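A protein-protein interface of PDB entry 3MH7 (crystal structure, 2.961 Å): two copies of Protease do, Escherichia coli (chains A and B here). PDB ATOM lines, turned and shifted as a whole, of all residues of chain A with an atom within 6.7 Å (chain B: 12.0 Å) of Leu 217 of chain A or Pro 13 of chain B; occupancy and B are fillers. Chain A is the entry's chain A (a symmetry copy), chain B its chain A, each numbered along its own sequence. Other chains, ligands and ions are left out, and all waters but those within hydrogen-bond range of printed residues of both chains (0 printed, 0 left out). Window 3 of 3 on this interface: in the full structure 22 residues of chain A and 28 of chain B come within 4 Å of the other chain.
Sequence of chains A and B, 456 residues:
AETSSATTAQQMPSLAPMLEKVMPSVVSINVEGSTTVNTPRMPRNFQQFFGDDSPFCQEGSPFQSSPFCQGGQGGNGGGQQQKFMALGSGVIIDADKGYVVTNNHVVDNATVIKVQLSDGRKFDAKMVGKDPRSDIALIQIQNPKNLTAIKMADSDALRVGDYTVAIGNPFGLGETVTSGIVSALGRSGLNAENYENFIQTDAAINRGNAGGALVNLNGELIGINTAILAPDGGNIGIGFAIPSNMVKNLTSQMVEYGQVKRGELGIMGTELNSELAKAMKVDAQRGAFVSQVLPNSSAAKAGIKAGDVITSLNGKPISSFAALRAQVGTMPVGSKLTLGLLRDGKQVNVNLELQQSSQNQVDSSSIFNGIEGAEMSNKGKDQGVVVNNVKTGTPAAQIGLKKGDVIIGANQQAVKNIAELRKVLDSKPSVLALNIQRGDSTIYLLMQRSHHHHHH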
ATOM      1  N   LEU A  15     -22.612 -17.366 -37.786  1.00  0.00           N
ATOM      2  CA  LEU A  15     -21.524 -16.873 -36.917  1.00  0.00           C
ATOM      3  C   LEU A  15     -20.124 -17.208 -37.467  1.00  0.00           C
ATOM      4  O   LEU A  15     -19.100 -16.920 -36.833  1.00  0.00           O
ATOM      5  CB  LEU A  15     -21.652 -17.432 -35.503  1.00  0.00           C
ATOM      6  CG  LEU A  15     -22.986 -17.172 -34.798  1.00  0.00           C
ATOM      7  CD1 LEU A  15     -23.217 -18.127 -33.631  1.00  0.00           C
ATOM      8  CD2 LEU A  15     -23.053 -15.761 -34.312  1.00  0.00           C
ATOM      9  N   MET A  18     -17.296 -14.409 -38.246  1.00  0.00           N
ATOM     10  CA  MET A  18     -16.741 -13.842 -37.021  1.00  0.00           C
ATOM     11  C   MET A  18     -15.826 -14.825 -36.297  1.00  0.00           C
ATOM     12  O   MET A  18     -14.710 -14.474 -35.889  1.00  0.00           O
ATOM     13  CB  MET A  18     -17.858 -13.360 -36.088  1.00  0.00           C
ATOM     14  CG  MET A  18     -17.379 -12.957 -34.707  1.00  0.00           C
ATOM     15  SD  MET A  18     -17.448 -14.450 -33.430  1.00  0.00           S
ATOM     16  CE  MET A  18     -19.331 -14.338 -32.960  1.00  0.00           C
ATOM     17  N   LEU A  19     -16.301 -16.054 -36.149  1.00  0.00           N
ATOM     18  CA  LEU A  19     -15.574 -17.049 -35.400  1.00  0.00           C
ATOM     19  C   LEU A  19     -14.229 -17.366 -36.025  1.00  0.00           C
ATOM     20  O   LEU A  19     -13.298 -17.823 -35.349  1.00  0.00           O
ATOM     21  CB  LEU A  19     -16.389 -18.314 -35.355  1.00  0.00           C
ATOM     22  CG  LEU A  19     -17.602 -18.183 -34.478  1.00  0.00           C
ATOM     23  CD1 LEU A  19     -18.630 -19.191 -34.876  1.00  0.00           C
ATOM     24  CD2 LEU A  19     -17.193 -18.371 -33.041  1.00  0.00           C
ATOM     25  N   GLY A 161     -31.070  -8.594 -23.256  1.00  0.00           N
ATOM     26  CA  GLY A 161     -31.390  -9.270 -24.520  1.00  0.00           C
ATOM     27  C   GLY A 161     -30.234  -9.828 -25.382  1.00  0.00           C
ATOM     28  O   GLY A 161     -30.457 -10.515 -26.364  1.00  0.00           O
ATOM     29  N   ASP A 162     -29.000  -9.510 -25.013  1.00  0.00           N
ATOM     30  CA  ASP A 162     -27.873  -9.566 -25.927  1.00  0.00           C
ATOM     31  C   ASP A 162     -27.413 -10.966 -26.335  1.00  0.00           C
ATOM     32  O   ASP A 162     -27.385 -11.887 -25.525  1.00  0.00           O
ATOM     33  CB  ASP A 162     -26.730  -8.739 -25.341  1.00  0.00           C
ATOM     34  CG  ASP A 162     -26.926  -7.233 -25.579  1.00  0.00           C
ATOM     35  OD1 ASP A 162     -27.955  -6.869 -26.205  1.00  0.00           O
ATOM     36  OD2 ASP A 162     -26.063  -6.414 -25.157  1.00  0.00           O
ATOM     37  N   TYR A 163     -27.050 -11.143 -27.599  1.00  0.00           N
ATOM     38  CA  TYR A 163     -26.611 -12.469 -28.036  1.00  0.00           C
ATOM     39  C   TYR A 163     -25.212 -12.772 -27.523  1.00  0.00           C
ATOM     40  O   TYR A 163     -24.380 -11.877 -27.444  1.00  0.00           O
ATOM     41  CB  TYR A 163     -26.676 -12.585 -29.565  1.00  0.00           C
ATOM     42  CG  TYR A 163     -28.086 -12.749 -30.031  1.00  0.00           C
ATOM     43  CD1 TYR A 163     -28.748 -11.730 -30.688  1.00  0.00           C
ATOM     44  CD2 TYR A 163     -28.778 -13.905 -29.752  1.00  0.00           C
ATOM     45  CE1 TYR A 163     -30.057 -11.871 -31.100  1.00  0.00           C
ATOM     46  CE2 TYR A 163     -30.072 -14.075 -30.153  1.00  0.00           C
ATOM     47  CZ  TYR A 163     -30.724 -13.057 -30.829  1.00  0.00           C
ATOM     48  OH  TYR A 163     -32.045 -13.255 -31.218  1.00  0.00           O
ATOM     49  N   THR A 164     -24.938 -14.019 -27.183  1.00  0.00           N
ATOM     50  CA  THR A 164     -23.599 -14.394 -26.764  1.00  0.00           C
ATOM     51  C   THR A 164     -23.156 -15.691 -27.423  1.00  0.00           C
ATOM     52  O   THR A 164     -23.960 -16.598 -27.636  1.00  0.00           O
ATOM     53  CB  THR A 164     -23.592 -14.674 -25.272  1.00  0.00           C
ATOM     54  OG1 THR A 164     -24.465 -15.785 -24.999  1.00  0.00           O
ATOM     55  CG2 THR A 164     -24.064 -13.456 -24.505  1.00  0.00           C
ATOM     56  N   VAL A 165     -21.873 -15.802 -27.732  1.00  0.00           N
ATOM     57  CA  VAL A 165     -21.332 -17.122 -28.072  1.00  0.00           C
ATOM     58  C   VAL A 165     -20.192 -17.499 -27.123  1.00  0.00           C
ATOM     59  O   VAL A 165     -19.376 -16.642 -26.739  1.00  0.00           O
ATOM     60  CB  VAL A 165     -20.932 -17.292 -29.580  1.00  0.00           C
ATOM     61  CG1 VAL A 165     -21.327 -16.089 -30.399  1.00  0.00           C
ATOM     62  CG2 VAL A 165     -19.466 -17.549 -29.717  1.00  0.00           C
ATOM     63  N   VAL A 215     -18.119 -14.220 -25.867  1.00  0.00           N
ATOM     64  CA  VAL A 215     -18.007 -13.076 -26.766  1.00  0.00           C
ATOM     65  C   VAL A 215     -19.358 -12.620 -27.326  1.00  0.00           C
ATOM     66  O   VAL A 215     -20.336 -13.350 -27.308  1.00  0.00           O
ATOM     67  CB  VAL A 215     -17.018 -13.364 -27.938  1.00  0.00           C
ATOM     68  CG1 VAL A 215     -15.894 -14.207 -27.435  1.00  0.00           C
ATOM     69  CG2 VAL A 215     -17.704 -14.074 -29.061  1.00  0.00           C
ATOM     70  N   ASN A 216     -19.407 -11.398 -27.816  1.00  0.00           N
ATOM     71  CA  ASN A 216     -20.599 -10.943 -28.495  1.00  0.00           C
ATOM     72  C   ASN A 216     -20.540 -11.231 -29.991  1.00  0.00           C
ATOM     73  O   ASN A 216     -19.582 -11.832 -30.469  1.00  0.00           O
ATOM     74  CB  ASN A 216     -20.833  -9.463 -28.245  1.00  0.00           C
ATOM     75  CG  ASN A 216     -19.694  -8.619 -28.712  1.00  0.00           C
ATOM     76  OD1 ASN A 216     -18.992  -8.982 -29.656  1.00  0.00           O
ATOM     77  ND2 ASN A 216     -19.490  -7.484 -28.056  1.00  0.00           N
ATOM     78  N   LEU A 217     -21.570 -10.812 -30.719  1.00  0.00           N
ATOM     79  CA  LEU A 217     -21.625 -11.114 -32.132  1.00  0.00           C
ATOM     80  C   LEU A 217     -20.451 -10.521 -32.939  1.00  0.00           C
ATOM     81  O   LEU A 217     -20.112 -11.023 -34.013  1.00  0.00           O
ATOM     82  CB  LEU A 217     -22.962 -10.697 -32.721  1.00  0.00           C
ATOM     83  CG  LEU A 217     -24.196 -11.522 -32.320  1.00  0.00           C
ATOM     84  CD1 LEU A 217     -25.464 -11.045 -33.074  1.00  0.00           C
ATOM     85  CD2 LEU A 217     -24.001 -13.045 -32.483  1.00  0.00           C
ATOM     86  N   ASN A 218     -19.813  -9.477 -32.428  1.00  0.00           N
ATOM     87  CA  ASN A 218     -18.658  -8.910 -33.114  1.00  0.00           C
ATOM     88  C   ASN A 218     -17.356  -9.580 -32.731  1.00  0.00           C
ATOM     89  O   ASN A 218     -16.288  -9.112 -33.067  1.00  0.00           O
ATOM     90  CB  ASN A 218     -18.560  -7.413 -32.848  1.00  0.00           C
ATOM     91  CG  ASN A 218     -19.530  -6.636 -33.682  1.00  0.00           C
ATOM     92  OD1 ASN A 218     -19.812  -7.029 -34.812  1.00  0.00           O
ATOM     93  ND2 ASN A 218     -20.066  -5.541 -33.143  1.00  0.00           N
ATOM     94  N   GLY A 219     -17.440 -10.669 -31.996  1.00  0.00           N
ATOM     95  CA  GLY A 219     -16.239 -11.342 -31.565  1.00  0.00           C
ATOM     96  C   GLY A 219     -15.422 -10.620 -30.508  1.00  0.00           C
ATOM     97  O   GLY A 219     -14.244 -10.956 -30.332  1.00  0.00           O
ATOM     98  N   GLU A 220     -16.000  -9.635 -29.817  1.00  0.00           N
ATOM     99  CA  GLU A 220     -15.294  -9.038 -28.690  1.00  0.00           C
ATOM    100  C   GLU A 220     -15.577  -9.810 -27.417  1.00  0.00           C
ATOM    101  O   GLU A 220     -16.696 -10.240 -27.152  1.00  0.00           O
ATOM    102  CB  GLU A 220     -15.697  -7.605 -28.464  1.00  0.00           C
ATOM    103  CG  GLU A 220     -15.138  -6.629 -29.422  1.00  0.00           C
ATOM    104  CD  GLU A 220     -16.121  -5.491 -29.713  1.00  0.00           C
ATOM    105  OE1 GLU A 220     -15.740  -4.616 -30.532  1.00  0.00           O
ATOM    106  OE2 GLU A 220     -17.265  -5.482 -29.148  1.00  0.00           O
ATOM    107  N   GLN B  11     -25.988  -1.567 -34.171  1.00  0.00           N
ATOM    108  CA  GLN B  11     -25.728  -2.381 -35.366  1.00  0.00           C
ATOM    109  C   GLN B  11     -25.729  -3.908 -35.118  1.00  0.00           C
ATOM    110  O   GLN B  11     -25.628  -4.704 -36.072  1.00  0.00           O
ATOM    111  CB  GLN B  11     -24.433  -1.932 -36.073  1.00  0.00           C
ATOM    112  CG  GLN B  11     -23.269  -1.550 -35.141  1.00  0.00           C
ATOM    113  CD  GLN B  11     -22.496  -2.749 -34.579  1.00  0.00           C
ATOM    114  OE1 GLN B  11     -22.015  -3.614 -35.333  1.00  0.00           O
ATOM    115  NE2 GLN B  11     -22.345  -2.783 -33.247  1.00  0.00           N
ATOM    116  N   MET B  12     -25.840  -4.303 -33.845  1.00  0.00           N
ATOM    117  CA  MET B  12     -26.004  -5.706 -33.463  1.00  0.00           C
ATOM    118  C   MET B  12     -27.477  -6.027 -33.141  1.00  0.00           C
ATOM    119  O   MET B  12     -28.116  -5.331 -32.347  1.00  0.00           O
ATOM    120  CB  MET B  12     -25.128  -6.039 -32.246  1.00  0.00           C
ATOM    121  CG  MET B  12     -23.625  -5.921 -32.468  1.00  0.00           C
ATOM    122  SD  MET B  12     -22.443  -6.791 -31.102  1.00  0.00           S
ATOM    123  CE  MET B  12     -22.862  -5.714 -29.535  1.00  0.00           C
ATOM    124  N   PRO B  13     -28.014  -7.097 -33.741  1.00  0.00           N
ATOM    125  CA  PRO B  13     -29.320  -7.614 -33.328  1.00  0.00           C
ATOM    126  C   PRO B  13     -29.364  -8.016 -31.838  1.00  0.00           C
ATOM    127  O   PRO B  13     -28.375  -8.558 -31.327  1.00  0.00           O
ATOM    128  CB  PRO B  13     -29.533  -8.836 -34.253  1.00  0.00           C
ATOM    129  CG  PRO B  13     -28.213  -9.158 -34.809  1.00  0.00           C
ATOM    130  CD  PRO B  13     -27.434  -7.874 -34.845  1.00  0.00           C
ATOM    131  N   SER B  14     -30.488  -7.750 -31.163  1.00  0.00           N
ATOM    132  CA  SER B  14     -30.648  -8.057 -29.744  1.00  0.00           C
ATOM    133  C   SER B  14     -32.098  -8.158 -29.283  1.00  0.00           C
ATOM    134  O   SER B  14     -32.953  -7.419 -29.763  1.00  0.00           O
ATOM    135  CB  SER B  14     -29.971  -6.984 -28.914  1.00  0.00           C
ATOM    136  OG  SER B  14     -30.233  -7.195 -27.532  1.00  0.00           O
ATOM    137  N   LEU B  15     -32.377  -9.049 -28.327  1.00  0.00           N
ATOM    138  CA  LEU B  15     -33.707  -9.069 -27.687  1.00  0.00           C
ATOM    139  C   LEU B  15     -33.872  -7.969 -26.620  1.00  0.00           C
ATOM    140  O   LEU B  15     -34.907  -7.881 -25.944  1.00  0.00           O
ATOM    141  CB  LEU B  15     -33.995 -10.426 -27.053  1.00  0.00           C
ATOM    142  CG  LEU B  15     -33.891 -11.636 -27.987  1.00  0.00           C
ATOM    143  CD1 LEU B  15     -33.723 -12.943 -27.218  1.00  0.00           C
ATOM    144  CD2 LEU B  15     -35.097 -11.723 -28.864  1.00  0.00           C
ATOM    145  N   ALA B  16     -32.857  -7.127 -26.466  1.00  0.00           N
ATOM    146  CA  ALA B  16     -32.811  -6.281 -25.303  1.00  0.00           C
ATOM    147  C   ALA B  16     -33.914  -5.216 -25.345  1.00  0.00           C
ATOM    148  O   ALA B  16     -34.699  -5.079 -24.403  1.00  0.00           O
ATOM    149  CB  ALA B  16     -31.445  -5.695 -25.151  1.00  0.00           C
ATOM    150  N   PRO B  17     -34.006  -4.481 -26.459  1.00  0.00           N
ATOM    151  CA  PRO B  17     -35.062  -3.463 -26.603  1.00  0.00           C
ATOM    152  C   PRO B  17     -36.453  -3.984 -26.243  1.00  0.00           C
ATOM    153  O   PRO B  17     -37.195  -3.322 -25.529  1.00  0.00           O
ATOM    154  CB  PRO B  17     -34.995  -3.113 -28.085  1.00  0.00           C
ATOM    155  CG  PRO B  17     -33.570  -3.372 -28.462  1.00  0.00           C
ATOM    156  CD  PRO B  17     -33.108  -4.532 -27.629  1.00  0.00           C
ATOM    157  N   MET B  18     -36.802  -5.168 -26.723  1.00  0.00           N
ATOM    158  CA  MET B  18     -38.110  -5.740 -26.418  1.00  0.00           C
ATOM    159  C   MET B  18     -38.252  -6.093 -24.940  1.00  0.00           C
ATOM    160  O   MET B  18     -39.256  -5.757 -24.298  1.00  0.00           O
ATOM    161  CB  MET B  18     -38.388  -6.968 -27.293  1.00  0.00           C
ATOM    162  CG  MET B  18     -39.626  -7.746 -26.892  1.00  0.00           C
ATOM    163  SD  MET B  18     -39.218  -9.190 -25.621  1.00  0.00           S
ATOM    164  CE  MET B  18     -38.620 -10.531 -26.895  1.00  0.00           C
ATOM    165  N   LEU B  19     -37.239  -6.763 -24.408  1.00  0.00           N
ATOM    166  CA  LEU B  19     -37.293  -7.237 -23.047  1.00  0.00           C
ATOM    167  C   LEU B  19     -37.404  -6.101 -22.049  1.00  0.00           C
ATOM    168  O   LEU B  19     -37.894  -6.278 -20.926  1.00  0.00           O
ATOM    169  CB  LEU B  19     -36.034  -8.010 -22.753  1.00  0.00           C
ATOM    170  CG  LEU B  19     -35.991  -9.328 -23.472  1.00  0.00           C
ATOM    171  CD1 LEU B  19     -34.575  -9.788 -23.608  1.00  0.00           C
ATOM    172  CD2 LEU B  19     -36.811 -10.334 -22.707  1.00  0.00           C
ATOM    173  N   TYR B 163     -39.871 -18.163 -33.116  1.00  0.00           N
ATOM    174  CA  TYR B 163     -38.933 -17.902 -32.025  1.00  0.00           C
ATOM    175  C   TYR B 163     -39.675 -17.664 -30.719  1.00  0.00           C
ATOM    176  O   TYR B 163     -40.749 -17.073 -30.722  1.00  0.00           O
ATOM    177  CB  TYR B 163     -38.021 -16.716 -32.366  1.00  0.00           C
ATOM    178  CG  TYR B 163     -36.972 -17.114 -33.353  1.00  0.00           C
ATOM    179  CD1 TYR B 163     -37.015 -16.674 -34.663  1.00  0.00           C
ATOM    180  CD2 TYR B 163     -35.972 -17.986 -32.989  1.00  0.00           C
ATOM    181  CE1 TYR B 163     -36.060 -17.057 -35.581  1.00  0.00           C
ATOM    182  CE2 TYR B 163     -35.011 -18.377 -33.876  1.00  0.00           C
ATOM    183  CZ  TYR B 163     -35.047 -17.917 -35.181  1.00  0.00           C
ATOM    184  OH  TYR B 163     -34.059 -18.339 -36.065  1.00  0.00           O
ATOM    185  N   VAL B 165     -39.088 -16.487 -26.401  1.00  0.00           N
ATOM    186  CA  VAL B 165     -38.254 -16.250 -25.217  1.00  0.00           C
ATOM    187  C   VAL B 165     -39.045 -16.520 -23.937  1.00  0.00           C
ATOM    188  O   VAL B 165     -40.244 -16.197 -23.850  1.00  0.00           O
ATOM    189  CB  VAL B 165     -37.543 -14.851 -25.194  1.00  0.00           C
ATOM    190  CG1 VAL B 165     -37.760 -14.095 -26.481  1.00  0.00           C
ATOM    191  CG2 VAL B 165     -38.010 -14.036 -24.032  1.00  0.00           C
ATOM    192  N   SER B 179     -33.960 -18.285 -24.323  1.00  0.00           N
ATOM    193  CA  SER B 179     -34.703 -18.340 -25.590  1.00  0.00           C
ATOM    194  C   SER B 179     -34.529 -19.619 -26.422  1.00  0.00           C
ATOM    195  O   SER B 179     -33.594 -20.399 -26.219  1.00  0.00           O
ATOM    196  CB  SER B 179     -34.338 -17.155 -26.471  1.00  0.00           C
ATOM    197  OG  SER B 179     -32.990 -17.302 -26.858  1.00  0.00           O
ATOM    198  N   LEU B 217     -41.155 -12.669 -30.281  1.00  0.00           N
ATOM    199  CA  LEU B 217     -40.178 -11.618 -30.463  1.00  0.00           C
ATOM    200  C   LEU B 217     -40.745 -10.200 -30.241  1.00  0.00           C
ATOM    201  O   LEU B 217     -39.999  -9.269 -29.929  1.00  0.00           O
ATOM    202  CB  LEU B 217     -39.507 -11.735 -31.821  1.00  0.00           C
ATOM    203  CG  LEU B 217     -38.536 -12.910 -32.027  1.00  0.00           C
ATOM    204  CD1 LEU B 217     -37.854 -12.840 -33.418  1.00  0.00           C
ATOM    205  CD2 LEU B 217     -37.484 -13.047 -30.906  1.00  0.00           C
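SD of Met 12 of chain B sits at hydrogen-bond distance from ND2 of Asn 218 of chain A (3.4 Å). O of Gly 161 of chain A lies within hydrogen-bond range of N of Leu 15 of chain B (3.1 Å). The side-chain hydroxyl (OG) of Ser 14 of chain B lies within hydrogen-bond range of the side-chain carboxylate (OD1) of Asp 162 of chain A.
The side-chain hydroxyl of Ser 14 of chain B sits at hydrogen-bond distance from the backbone NH of Ala 16 of chain B (2.8 Å). The side-chain amide oxygen of Asn 216 of chain A lies within hydrogen-bond range of the backbone NH of Asn 218 of chain A.
Ser 14 of chain B touches Gly 161 of chain A. Ala 16 of chain B touches Gly 161 of chain A (N to CA, 3.2 Å). Gly 161 of chain A touches Leu 19 of chain B. Asp 162 of chain A touches Ala 16 of chain B (OD1 to CB, 3.8 Å). Pro 13 of chain B touches Tyr 163 of chain A (O to CD1, 3.3 Å). CD1 of Leu 217 of chain A touches CG of Pro 13 of chain B, 3.8 Å away. OE1 of Gln 11 of chain B touches ND2 of Asn 218 of chain A (3.5 Å).
Printed residues of chain B within 4 Å of Leu 217 of chain A: Pro 13 (3.8 Å). No residue of chain B comes within 4 Å of Leu 15 of chain A. Asp 162 of chain A touches two residues of chain B. Of chain B, only Pro 13 comes within 4 Å of Tyr 163 of chain A. No residue of chain B comes within 4 Å of Val 165 of chain A. No residue of chain B comes within 4 Å of Val 215 of chain A. Gly 219 of chain A touches none of the printed residues of chain B. No residue of chain B comes within 4 Å of Glu 220 of chain A. Of the printed residues of chain A, Gln 11 of chain B touches Asn 218. Printed residues of chain A within 4 Å of Ser 14 of chain B: Gly 161 and Asp 162. Tyr 163 of chain B touches none of the printed residues of chain A. Leu 19 of chain A touches none of the printed residues of chain B. The nearest residue of chain A that does not touch Pro 13 of chain B is Asp 162 of chain A (5.4 Å).
Printed residues of chain A that touch a printed residue of chain B: Gly 161, Asp 162, Tyr 163, Leu 217 and Asn 218. Hydrophobic or aromatic side chains of chain A that line the printed part of chain B: Tyr 163 and Leu 217.
6 positions are printed for both chains. Of the 10 pairs that touch across the chains among the printed residues, none has its exchanged pair printed and touching as well.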
